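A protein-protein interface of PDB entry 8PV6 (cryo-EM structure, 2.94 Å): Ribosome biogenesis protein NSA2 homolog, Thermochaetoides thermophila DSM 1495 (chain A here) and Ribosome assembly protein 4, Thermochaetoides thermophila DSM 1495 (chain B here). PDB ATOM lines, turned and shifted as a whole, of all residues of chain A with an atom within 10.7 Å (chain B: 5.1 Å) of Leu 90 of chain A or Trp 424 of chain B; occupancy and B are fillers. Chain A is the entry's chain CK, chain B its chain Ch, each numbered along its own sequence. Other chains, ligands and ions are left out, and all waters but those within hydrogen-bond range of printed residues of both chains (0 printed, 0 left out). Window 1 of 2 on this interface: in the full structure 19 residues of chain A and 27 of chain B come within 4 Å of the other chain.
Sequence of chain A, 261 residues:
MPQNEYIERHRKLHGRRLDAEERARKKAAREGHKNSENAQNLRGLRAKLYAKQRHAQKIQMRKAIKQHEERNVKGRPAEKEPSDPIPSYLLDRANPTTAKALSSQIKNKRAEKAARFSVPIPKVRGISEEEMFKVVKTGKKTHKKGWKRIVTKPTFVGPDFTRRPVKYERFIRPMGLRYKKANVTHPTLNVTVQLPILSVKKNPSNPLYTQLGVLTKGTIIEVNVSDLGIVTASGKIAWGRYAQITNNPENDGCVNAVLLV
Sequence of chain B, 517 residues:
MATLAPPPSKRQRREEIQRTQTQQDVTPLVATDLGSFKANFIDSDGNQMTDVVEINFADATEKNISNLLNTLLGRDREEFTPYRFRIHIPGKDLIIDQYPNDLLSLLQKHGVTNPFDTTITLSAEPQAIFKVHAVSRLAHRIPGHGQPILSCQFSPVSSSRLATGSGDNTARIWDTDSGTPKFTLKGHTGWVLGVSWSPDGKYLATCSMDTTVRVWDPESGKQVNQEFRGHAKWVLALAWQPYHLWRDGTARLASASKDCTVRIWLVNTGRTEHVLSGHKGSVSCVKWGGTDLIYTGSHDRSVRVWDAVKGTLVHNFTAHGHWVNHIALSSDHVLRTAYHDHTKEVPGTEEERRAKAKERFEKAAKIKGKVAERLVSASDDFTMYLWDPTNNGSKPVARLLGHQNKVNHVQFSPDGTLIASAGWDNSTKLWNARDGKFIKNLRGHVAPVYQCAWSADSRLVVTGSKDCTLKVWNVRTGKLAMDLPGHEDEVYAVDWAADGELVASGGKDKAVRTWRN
O of Pro 85 of chain A touches CE2 of Tyr 492 of chain B, 3.99 Å away.
Pro 87 of chain A touches Tyr 492 of chain B (CG to CG, 3.5 Å).
Tyr 89 of chain A touches Asn 408 of chain B.
Tyr 450 of chain B touches Tyr 89 of chain A.
Trp 424 of chain B touches Leu 90 of chain A (CZ2 to CD2, 3.7 Å).
Tyr 450 of chain B touches Leu 90 of chain A.
CD1 of Leu 90 of chain A touches CE1 of Tyr 492 of chain B, 3.9 Å away.
Arg 93 of chain A touches Lys 406 of chain B (NH1 to CD, 3.8 Å).
OH of Tyr 89 of chain A is in hydrogen-bond range of O of Tyr 492 of chain B, at 2.5 Å.
The side-chain amide oxygen (OD1) of Asn 405 of chain B sits at hydrogen-bond distance from the side-chain amino group (NZ) of Lys 406 of chain B, 3.5 Å away.
The side-chain amide nitrogen (ND2) of Asn 405 of chain B sits at hydrogen-bond distance from the backbone carbonyl oxygen (O) of Trp 424 of chain B (3.4 Å).
The backbone NH (N) of Asn 408 of chain B sits at hydrogen-bond distance from the backbone carbonyl oxygen (O) of Ala 422 of chain B (3.0 Å).
N of Trp 424 of chain B sits at hydrogen-bond distance from O of Lys 406 of chain B (2.6 Å).
NE1 of Trp 424 of chain B sits at hydrogen-bond distance from OD1 of Asn 408 of chain B.
The side-chain amide nitrogen (ND2) of Asn 408 of chain B sits at hydrogen-bond distance from the backbone carbonyl oxygen (O) of Tyr 450 of chain B (3.0 Å).
Of the printed residues of chain B, Leu 90 of chain A touches Trp 424 (3.7 Å), Tyr 450 (3.99 Å) and Tyr 492 (3.9 Å).
Of the printed residues of chain A, Trp 424 of chain B touches Leu 90.
No residue of chain A comes within 4 Å of Asn 405 of chain B.
Of chain A, only Arg 93 (3.8 Å) comes within 4 Å of Lys 406 of chain B.
Val 407 of chain B touches none of the printed residues of chain A.
Of chain A, only Tyr 89 comes within 4 Å of Asn 408 of chain B.
Gly 423 of chain B touches none of the printed residues of chain A.
Asp 425 of chain B touches none of the printed residues of chain A.
Of the printed residues of chain A, Tyr 492 of chain B touches Pro 85, Pro 87, Tyr 89 and Leu 90.
Of the printed residues of chain B, Arg 93 of chain A touches Lys 406.
Of the printed residues of chain B, Pro 85 of chain A touches Tyr 492 (3.99 Å).
Ser 83 of chain A touches none of the printed residues of chain B.
Ala 94 of chain A touches none of the printed residues of chain B.
The nearest printed residue of chain B that does not touch Leu 90 of chain A is Asn 408 of chain B (5.3 Å).
The nearest residue of chain A that does not touch Trp 424 of chain B is Arg 93 of chain A (4.4 Å).
Of the 13 printed residues of chain B, 5 touch a printed residue of chain A.
Printed residues of chain A that touch a printed residue of chain B: Pro 85, Pro 87, Tyr 89, Leu 90 and Arg 93.
Hydrophobic or aromatic side chains of chain A within 4 Å of the printed part of chain B: Pro 87, Tyr 89 and Leu 90.
Among the printed residues, 9 pairs touch across the chains.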
ATOM      1  N   PRO A  82      -9.454 -35.832 -19.567  1.00  0.00           N
ATOM      2  CA  PRO A  82      -8.000 -35.929 -19.401  1.00  0.00           C
ATOM      3  C   PRO A  82      -7.619 -36.566 -18.072  1.00  0.00           C
ATOM      4  O   PRO A  82      -8.462 -36.867 -17.225  1.00  0.00           O
ATOM      5  CB  PRO A  82      -7.532 -34.471 -19.478  1.00  0.00           C
ATOM      6  CG  PRO A  82      -8.722 -33.663 -19.110  1.00  0.00           C
ATOM      7  CD  PRO A  82      -9.923 -34.435 -19.575  1.00  0.00           C
ATOM      8  N   SER A  83      -6.313 -36.775 -17.899  1.00  0.00           N
ATOM      9  CA  SER A  83      -5.824 -37.471 -16.712  1.00  0.00           C
ATOM     10  C   SER A  83      -5.647 -36.516 -15.538  1.00  0.00           C
ATOM     11  O   SER A  83      -6.126 -36.782 -14.430  1.00  0.00           O
ATOM     12  CB  SER A  83      -4.508 -38.181 -17.029  1.00  0.00           C
ATOM     13  OG  SER A  83      -3.954 -38.771 -15.866  1.00  0.00           O
ATOM     14  N   ASP A  84      -4.953 -35.403 -15.759  1.00  0.00           N
ATOM     15  CA  ASP A  84      -4.602 -34.496 -14.677  1.00  0.00           C
ATOM     16  C   ASP A  84      -5.758 -33.526 -14.488  1.00  0.00           C
ATOM     17  O   ASP A  84      -6.209 -32.923 -15.475  1.00  0.00           O
ATOM     18  CB  ASP A  84      -3.309 -33.757 -15.033  1.00  0.00           C
ATOM     19  CG  ASP A  84      -2.826 -32.755 -13.963  1.00  0.00           C
ATOM     20  OD1 ASP A  84      -3.564 -32.289 -13.066  1.00  0.00           O
ATOM     21  OD2 ASP A  84      -1.624 -32.426 -14.044  1.00  0.00           O
ATOM     22  N   PRO A  85      -6.273 -33.348 -13.262  1.00  0.00           N
ATOM     23  CA  PRO A  85      -7.343 -32.365 -13.041  1.00  0.00           C
ATOM     24  C   PRO A  85      -6.900 -30.929 -13.278  1.00  0.00           C
ATOM     25  O   PRO A  85      -5.965 -30.437 -12.640  1.00  0.00           O
ATOM     26  CB  PRO A  85      -7.726 -32.591 -11.573  1.00  0.00           C
ATOM     27  CG  PRO A  85      -7.314 -33.990 -11.290  1.00  0.00           C
ATOM     28  CD  PRO A  85      -6.060 -34.200 -12.082  1.00  0.00           C
ATOM     29  N   ILE A  86      -7.579 -30.256 -14.196  1.00  0.00           N
ATOM     30  CA  ILE A  86      -7.266 -28.885 -14.587  1.00  0.00           C
ATOM     31  C   ILE A  86      -8.556 -28.079 -14.507  1.00  0.00           C
ATOM     32  O   ILE A  86      -9.658 -28.643 -14.617  1.00  0.00           O
ATOM     33  CB  ILE A  86      -6.623 -28.825 -15.993  1.00  0.00           C
ATOM     34  CG1 ILE A  86      -7.589 -29.363 -17.049  1.00  0.00           C
ATOM     35  CG2 ILE A  86      -5.299 -29.567 -16.027  1.00  0.00           C
ATOM     36  CD1 ILE A  86      -7.129 -29.128 -18.465  1.00  0.00           C
ATOM     37  N   PRO A  87      -8.467 -26.765 -14.292  1.00  0.00           N
ATOM     38  CA  PRO A  87      -9.686 -25.952 -14.179  1.00  0.00           C
ATOM     39  C   PRO A  87     -10.399 -25.795 -15.516  1.00  0.00           C
ATOM     40  O   PRO A  87      -9.977 -26.301 -16.557  1.00  0.00           O
ATOM     41  CB  PRO A  87      -9.186 -24.600 -13.662  1.00  0.00           C
ATOM     42  CG  PRO A  87      -7.829 -24.845 -13.151  1.00  0.00           C
ATOM     43  CD  PRO A  87      -7.268 -25.993 -13.915  1.00  0.00           C
ATOM     44  N   SER A  88     -11.512 -25.060 -15.465  1.00  0.00           N
ATOM     45  CA  SER A  88     -12.374 -24.923 -16.632  1.00  0.00           C
ATOM     46  C   SER A  88     -11.746 -24.049 -17.710  1.00  0.00           C
ATOM     47  O   SER A  88     -12.018 -24.242 -18.900  1.00  0.00           O
ATOM     48  CB  SER A  88     -13.730 -24.357 -16.216  1.00  0.00           C
ATOM     49  OG  SER A  88     -13.585 -23.080 -15.622  1.00  0.00           O
ATOM     50  N   TYR A  89     -10.910 -23.086 -17.325  1.00  0.00           N
ATOM     51  CA  TYR A  89     -10.285 -22.216 -18.313  1.00  0.00           C
ATOM     52  C   TYR A  89      -9.088 -22.857 -18.999  1.00  0.00           C
ATOM     53  O   TYR A  89      -8.597 -22.306 -19.989  1.00  0.00           O
ATOM     54  CB  TYR A  89      -9.879 -20.883 -17.669  1.00  0.00           C
ATOM     55  CG  TYR A  89      -9.028 -20.988 -16.418  1.00  0.00           C
ATOM     56  CD1 TYR A  89      -7.655 -21.180 -16.496  1.00  0.00           C
ATOM     57  CD2 TYR A  89      -9.601 -20.875 -15.160  1.00  0.00           C
ATOM     58  CE1 TYR A  89      -6.882 -21.270 -15.357  1.00  0.00           C
ATOM     59  CE2 TYR A  89      -8.834 -20.962 -14.016  1.00  0.00           C
ATOM     60  CZ  TYR A  89      -7.477 -21.160 -14.122  1.00  0.00           C
ATOM     61  OH  TYR A  89      -6.710 -21.247 -12.985  1.00  0.00           O
ATOM     62  N   LEU A  90      -8.607 -23.999 -18.508  1.00  0.00           N
ATOM     63  CA  LEU A  90      -7.506 -24.716 -19.134  1.00  0.00           C
ATOM     64  C   LEU A  90      -7.974 -25.917 -19.944  1.00  0.00           C
ATOM     65  O   LEU A  90      -7.148 -26.595 -20.561  1.00  0.00           O
ATOM     66  CB  LEU A  90      -6.495 -25.164 -18.078  1.00  0.00           C
ATOM     67  CG  LEU A  90      -5.657 -24.053 -17.452  1.00  0.00           C
ATOM     68  CD1 LEU A  90      -4.717 -24.618 -16.405  1.00  0.00           C
ATOM     69  CD2 LEU A  90      -4.886 -23.315 -18.528  1.00  0.00           C
ATOM     70  N   LEU A  91      -9.275 -26.191 -19.960  1.00  0.00           N
ATOM     71  CA  LEU A  91      -9.798 -27.322 -20.706  1.00  0.00           C
ATOM     72  C   LEU A  91      -9.757 -27.046 -22.206  1.00  0.00           C
ATOM     73  O   LEU A  91      -9.698 -25.897 -22.653  1.00  0.00           O
ATOM     74  CB  LEU A  91     -11.229 -27.640 -20.271  1.00  0.00           C
ATOM     75  CG  LEU A  91     -11.374 -28.292 -18.897  1.00  0.00           C
ATOM     76  CD1 LEU A  91     -12.825 -28.295 -18.457  1.00  0.00           C
ATOM     77  CD2 LEU A  91     -10.821 -29.704 -18.925  1.00  0.00           C
ATOM     78  N   ASP A  92      -9.768 -28.134 -22.979  1.00  0.00           N
ATOM     79  CA  ASP A  92      -9.735 -28.155 -24.441  1.00  0.00           C
ATOM     80  C   ASP A  92      -8.507 -27.469 -25.022  1.00  0.00           C
ATOM     81  O   ASP A  92      -8.550 -27.007 -26.169  1.00  0.00           O
ATOM     82  CB  ASP A  92     -11.001 -27.539 -25.051  1.00  0.00           C
ATOM     83  CG  ASP A  92     -12.234 -28.387 -24.813  1.00  0.00           C
ATOM     84  OD1 ASP A  92     -12.092 -29.623 -24.701  1.00  0.00           O
ATOM     85  OD2 ASP A  92     -13.344 -27.820 -24.741  1.00  0.00           O
ATOM     86  N   ARG A  93      -7.412 -27.392 -24.273  1.00  0.00           N
ATOM     87  CA  ARG A  93      -6.171 -26.799 -24.743  1.00  0.00           C
ATOM     88  C   ARG A  93      -5.091 -27.868 -24.849  1.00  0.00           C
ATOM     89  O   ARG A  93      -5.187 -28.943 -24.252  1.00  0.00           O
ATOM     90  CB  ARG A  93      -5.705 -25.677 -23.811  1.00  0.00           C
ATOM     91  CG  ARG A  93      -6.719 -24.564 -23.620  1.00  0.00           C
ATOM     92  CD  ARG A  93      -6.158 -23.459 -22.744  1.00  0.00           C
ATOM     93  NE  ARG A  93      -7.131 -22.400 -22.507  1.00  0.00           N
ATOM     94  CZ  ARG A  93      -7.293 -21.342 -23.291  1.00  0.00           C
ATOM     95  NH1 ARG A  93      -6.568 -21.176 -24.384  1.00  0.00           N
ATOM     96  NH2 ARG A  93      -8.205 -20.431 -22.969  1.00  0.00           N
ATOM     97  N   ALA A  94      -4.057 -27.557 -25.622  1.00  0.00           N
ATOM     98  CA  ALA A  94      -2.945 -28.479 -25.814  1.00  0.00           C
ATOM     99  C   ALA A  94      -2.065 -28.536 -24.571  1.00  0.00           C
ATOM    100  O   ALA A  94      -1.615 -29.607 -24.166  1.00  0.00           O
ATOM    101  CB  ALA A  94      -2.126 -28.075 -27.027  1.00  0.00           C
ATOM    102  N   THR A 188      -6.648 -24.418 -33.742  1.00  0.00           N
ATOM    103  CA  THR A 188      -7.227 -24.228 -32.418  1.00  0.00           C
ATOM    104  C   THR A 188      -8.709 -23.883 -32.500  1.00  0.00           C
ATOM    105  O   THR A 188      -9.512 -24.397 -31.714  1.00  0.00           O
ATOM    106  CB  THR A 188      -6.463 -23.140 -31.664  1.00  0.00           C
ATOM    107  OG1 THR A 188      -5.057 -23.396 -31.760  1.00  0.00           O
ATOM    108  CG2 THR A 188      -6.860 -23.136 -30.200  1.00  0.00           C
ATOM    109  N   ASN B 405      -0.352 -11.775 -25.302  1.00  0.00           N
ATOM    110  CA  ASN B 405      -0.695 -13.190 -25.271  1.00  0.00           C
ATOM    111  C   ASN B 405      -2.167 -13.291 -24.890  1.00  0.00           C
ATOM    112  O   ASN B 405      -2.881 -12.287 -24.842  1.00  0.00           O
ATOM    113  CB  ASN B 405       0.208 -13.968 -24.313  1.00  0.00           C
ATOM    114  CG  ASN B 405       0.415 -15.406 -24.748  1.00  0.00           C
ATOM    115  OD1 ASN B 405      -0.401 -15.966 -25.478  1.00  0.00           O
ATOM    116  ND2 ASN B 405       1.512 -16.008 -24.306  1.00  0.00           N
ATOM    117  N   LYS B 406      -2.625 -14.518 -24.649  1.00  0.00           N
ATOM    118  CA  LYS B 406      -4.030 -14.740 -24.333  1.00  0.00           C
ATOM    119  C   LYS B 406      -4.384 -14.123 -22.987  1.00  0.00           C
ATOM    120  O   LYS B 406      -3.580 -14.126 -22.052  1.00  0.00           O
ATOM    121  CB  LYS B 406      -4.344 -16.235 -24.324  1.00  0.00           C
ATOM    122  CG  LYS B 406      -3.900 -16.967 -25.576  1.00  0.00           C
ATOM    123  CD  LYS B 406      -4.171 -18.456 -25.470  1.00  0.00           C
ATOM    124  CE  LYS B 406      -3.304 -19.105 -24.410  1.00  0.00           C
ATOM    125  NZ  LYS B 406      -1.864 -19.048 -24.778  1.00  0.00           N
ATOM    126  N   VAL B 407      -5.591 -13.575 -22.897  1.00  0.00           N
ATOM    127  CA  VAL B 407      -6.084 -12.972 -21.667  1.00  0.00           C
ATOM    128  C   VAL B 407      -6.991 -13.986 -20.989  1.00  0.00           C
ATOM    129  O   VAL B 407      -7.989 -14.426 -21.572  1.00  0.00           O
ATOM    130  CB  VAL B 407      -6.831 -11.658 -21.938  1.00  0.00           C
ATOM    131  CG1 VAL B 407      -7.282 -11.042 -20.631  1.00  0.00           C
ATOM    132  CG2 VAL B 407      -5.955 -10.700 -22.718  1.00  0.00           C
ATOM    133  N   ASN B 408      -6.649 -14.362 -19.760  1.00  0.00           N
ATOM    134  CA  ASN B 408      -7.362 -15.432 -19.078  1.00  0.00           C
ATOM    135  C   ASN B 408      -8.496 -14.923 -18.199  1.00  0.00           C
ATOM    136  O   ASN B 408      -9.595 -15.485 -18.224  1.00  0.00           O
ATOM    137  CB  ASN B 408      -6.387 -16.252 -18.233  1.00  0.00           C
ATOM    138  CG  ASN B 408      -6.899 -17.641 -17.945  1.00  0.00           C
ATOM    139  OD1 ASN B 408      -7.022 -18.468 -18.846  1.00  0.00           O
ATOM    140  ND2 ASN B 408      -7.214 -17.906 -16.683  1.00  0.00           N
ATOM    141  N   ALA B 422      -5.626 -10.256 -16.193  1.00  0.00           N
ATOM    142  CA  ALA B 422      -4.459 -11.111 -16.035  1.00  0.00           C
ATOM    143  C   ALA B 422      -4.265 -11.913 -17.312  1.00  0.00           C
ATOM    144  O   ALA B 422      -5.172 -12.640 -17.728  1.00  0.00           O
ATOM    145  CB  ALA B 422      -4.628 -12.047 -14.840  1.00  0.00           C
ATOM    146  N   GLY B 423      -3.086 -11.792 -17.932  1.00  0.00           N
ATOM    147  CA  GLY B 423      -2.846 -12.402 -19.218  1.00  0.00           C
ATOM    148  C   GLY B 423      -1.823 -13.518 -19.129  1.00  0.00           C
ATOM    149  O   GLY B 423      -1.209 -13.754 -18.088  1.00  0.00           O
ATOM    150  N   TRP B 424      -1.656 -14.207 -20.256  1.00  0.00           N
ATOM    151  CA  TRP B 424      -0.646 -15.246 -20.399  1.00  0.00           C
ATOM    152  C   TRP B 424       0.718 -14.683 -20.763  1.00  0.00           C
ATOM    153  O   TRP B 424       1.666 -15.453 -20.942  1.00  0.00           O
ATOM    154  CB  TRP B 424      -1.080 -16.273 -21.449  1.00  0.00           C
ATOM    155  CG  TRP B 424      -2.191 -17.184 -21.009  1.00  0.00           C
ATOM    156  CD1 TRP B 424      -3.414 -16.820 -20.529  1.00  0.00           C
ATOM    157  CD2 TRP B 424      -2.175 -18.615 -21.020  1.00  0.00           C
ATOM    158  NE1 TRP B 424      -4.160 -17.934 -20.237  1.00  0.00           N
ATOM    159  CE2 TRP B 424      -3.422 -19.049 -20.529  1.00  0.00           C
ATOM    160  CE3 TRP B 424      -1.228 -19.571 -21.393  1.00  0.00           C
ATOM    161  CZ2 TRP B 424      -3.744 -20.396 -20.403  1.00  0.00           C
ATOM    162  CZ3 TRP B 424      -1.550 -20.907 -21.267  1.00  0.00           C
ATOM    163  CH2 TRP B 424      -2.797 -21.308 -20.776  1.00  0.00           C
ATOM    164  N   ASP B 425       0.830 -13.360 -20.881  1.00  0.00           N
ATOM    165  CA  ASP B 425       2.088 -12.685 -21.158  1.00  0.00           C
ATOM    166  C   ASP B 425       2.788 -12.228 -19.884  1.00  0.00           C
ATOM    167  O   ASP B 425       3.449 -11.184 -19.891  1.00  0.00           O
ATOM    168  CB  ASP B 425       1.857 -11.498 -22.091  1.00  0.00           C
ATOM    169  CG  ASP B 425       0.755 -10.581 -21.603  1.00  0.00           C
ATOM    170  OD1 ASP B 425       0.039 -10.962 -20.655  1.00  0.00           O
ATOM    171  OD2 ASP B 425       0.605  -9.476 -22.165  1.00  0.00           O
ATOM    172  N   ASN B 426       2.618 -12.977 -18.792  1.00  0.00           N
ATOM    173  CA  ASN B 426       3.277 -12.774 -17.504  1.00  0.00           C
ATOM    174  C   ASN B 426       2.934 -11.436 -16.863  1.00  0.00           C
ATOM    175  O   ASN B 426       3.747 -10.889 -16.112  1.00  0.00           O
ATOM    176  CB  ASN B 426       4.802 -12.897 -17.623  1.00  0.00           C
ATOM    177  CG  ASN B 426       5.235 -14.197 -18.257  1.00  0.00           C
ATOM    178  OD1 ASN B 426       4.639 -15.241 -18.028  1.00  0.00           O
ATOM    179  ND2 ASN B 426       6.290 -14.138 -19.057  1.00  0.00           N
ATOM    180  N   PRO B 448       2.529 -17.620 -16.912  1.00  0.00           N
ATOM    181  CA  PRO B 448       1.224 -16.984 -17.160  1.00  0.00           C
ATOM    182  C   PRO B 448       0.352 -16.802 -15.928  1.00  0.00           C
ATOM    183  O   PRO B 448       0.205 -17.717 -15.113  1.00  0.00           O
ATOM    184  CB  PRO B 448       0.562 -17.948 -18.150  1.00  0.00           C
ATOM    185  CG  PRO B 448       1.689 -18.506 -18.917  1.00  0.00           C
ATOM    186  CD  PRO B 448       2.866 -18.583 -17.978  1.00  0.00           C
ATOM    187  N   VAL B 449      -0.228 -15.614 -15.789  1.00  0.00           N
ATOM    188  CA  VAL B 449      -1.036 -15.263 -14.629  1.00  0.00           C
ATOM    189  C   VAL B 449      -2.436 -15.807 -14.858  1.00  0.00           C
ATOM    190  O   VAL B 449      -3.090 -15.464 -15.849  1.00  0.00           O
ATOM    191  CB  VAL B 449      -1.059 -13.746 -14.397  1.00  0.00           C
ATOM    192  CG1 VAL B 449      -1.723 -13.429 -13.072  1.00  0.00           C
ATOM    193  CG2 VAL B 449       0.349 -13.184 -14.440  1.00  0.00           C
ATOM    194  N   TYR B 450      -2.898 -16.660 -13.947  1.00  0.00           N
ATOM    195  CA  TYR B 450      -4.180 -17.316 -14.141  1.00  0.00           C
ATOM    196  C   TYR B 450      -5.352 -16.522 -13.588  1.00  0.00           C
ATOM    197  O   TYR B 450      -6.350 -16.353 -14.295  1.00  0.00           O
ATOM    198  CB  TYR B 450      -4.163 -18.715 -13.525  1.00  0.00           C
ATOM    199  CG  TYR B 450      -3.410 -19.722 -14.362  1.00  0.00           C
ATOM    200  CD1 TYR B 450      -3.433 -19.650 -15.747  1.00  0.00           C
ATOM    201  CD2 TYR B 450      -2.687 -20.747 -13.772  1.00  0.00           C
ATOM    202  CE1 TYR B 450      -2.751 -20.564 -16.519  1.00  0.00           C
ATOM    203  CE2 TYR B 450      -2.003 -21.668 -14.537  1.00  0.00           C
ATOM    204  CZ  TYR B 450      -2.039 -21.571 -15.911  1.00  0.00           C
ATOM    205  OH  TYR B 450      -1.358 -22.486 -16.679  1.00  0.00           O
ATOM    206  N   TYR B 492      -4.260 -22.395  -9.143  1.00  0.00           N
ATOM    207  CA  TYR B 492      -5.421 -22.445 -10.021  1.00  0.00           C
ATOM    208  C   TYR B 492      -6.538 -21.495  -9.627  1.00  0.00           C
ATOM    209  O   TYR B 492      -7.145 -20.884 -10.507  1.00  0.00           O
ATOM    210  CB  TYR B 492      -5.988 -23.868 -10.071  1.00  0.00           C
ATOM    211  CG  TYR B 492      -5.157 -24.845 -10.869  1.00  0.00           C
ATOM    212  CD1 TYR B 492      -4.449 -24.433 -11.989  1.00  0.00           C
ATOM    213  CD2 TYR B 492      -5.090 -26.182 -10.508  1.00  0.00           C
ATOM    214  CE1 TYR B 492      -3.691 -25.326 -12.721  1.00  0.00           C
ATOM    215  CE2 TYR B 492      -4.337 -27.081 -11.232  1.00  0.00           C
ATOM    216  CZ  TYR B 492      -3.639 -26.648 -12.337  1.00  0.00           C
ATOM    217  OH  TYR B 492      -2.888 -27.545 -13.060  1.00  0.00           O
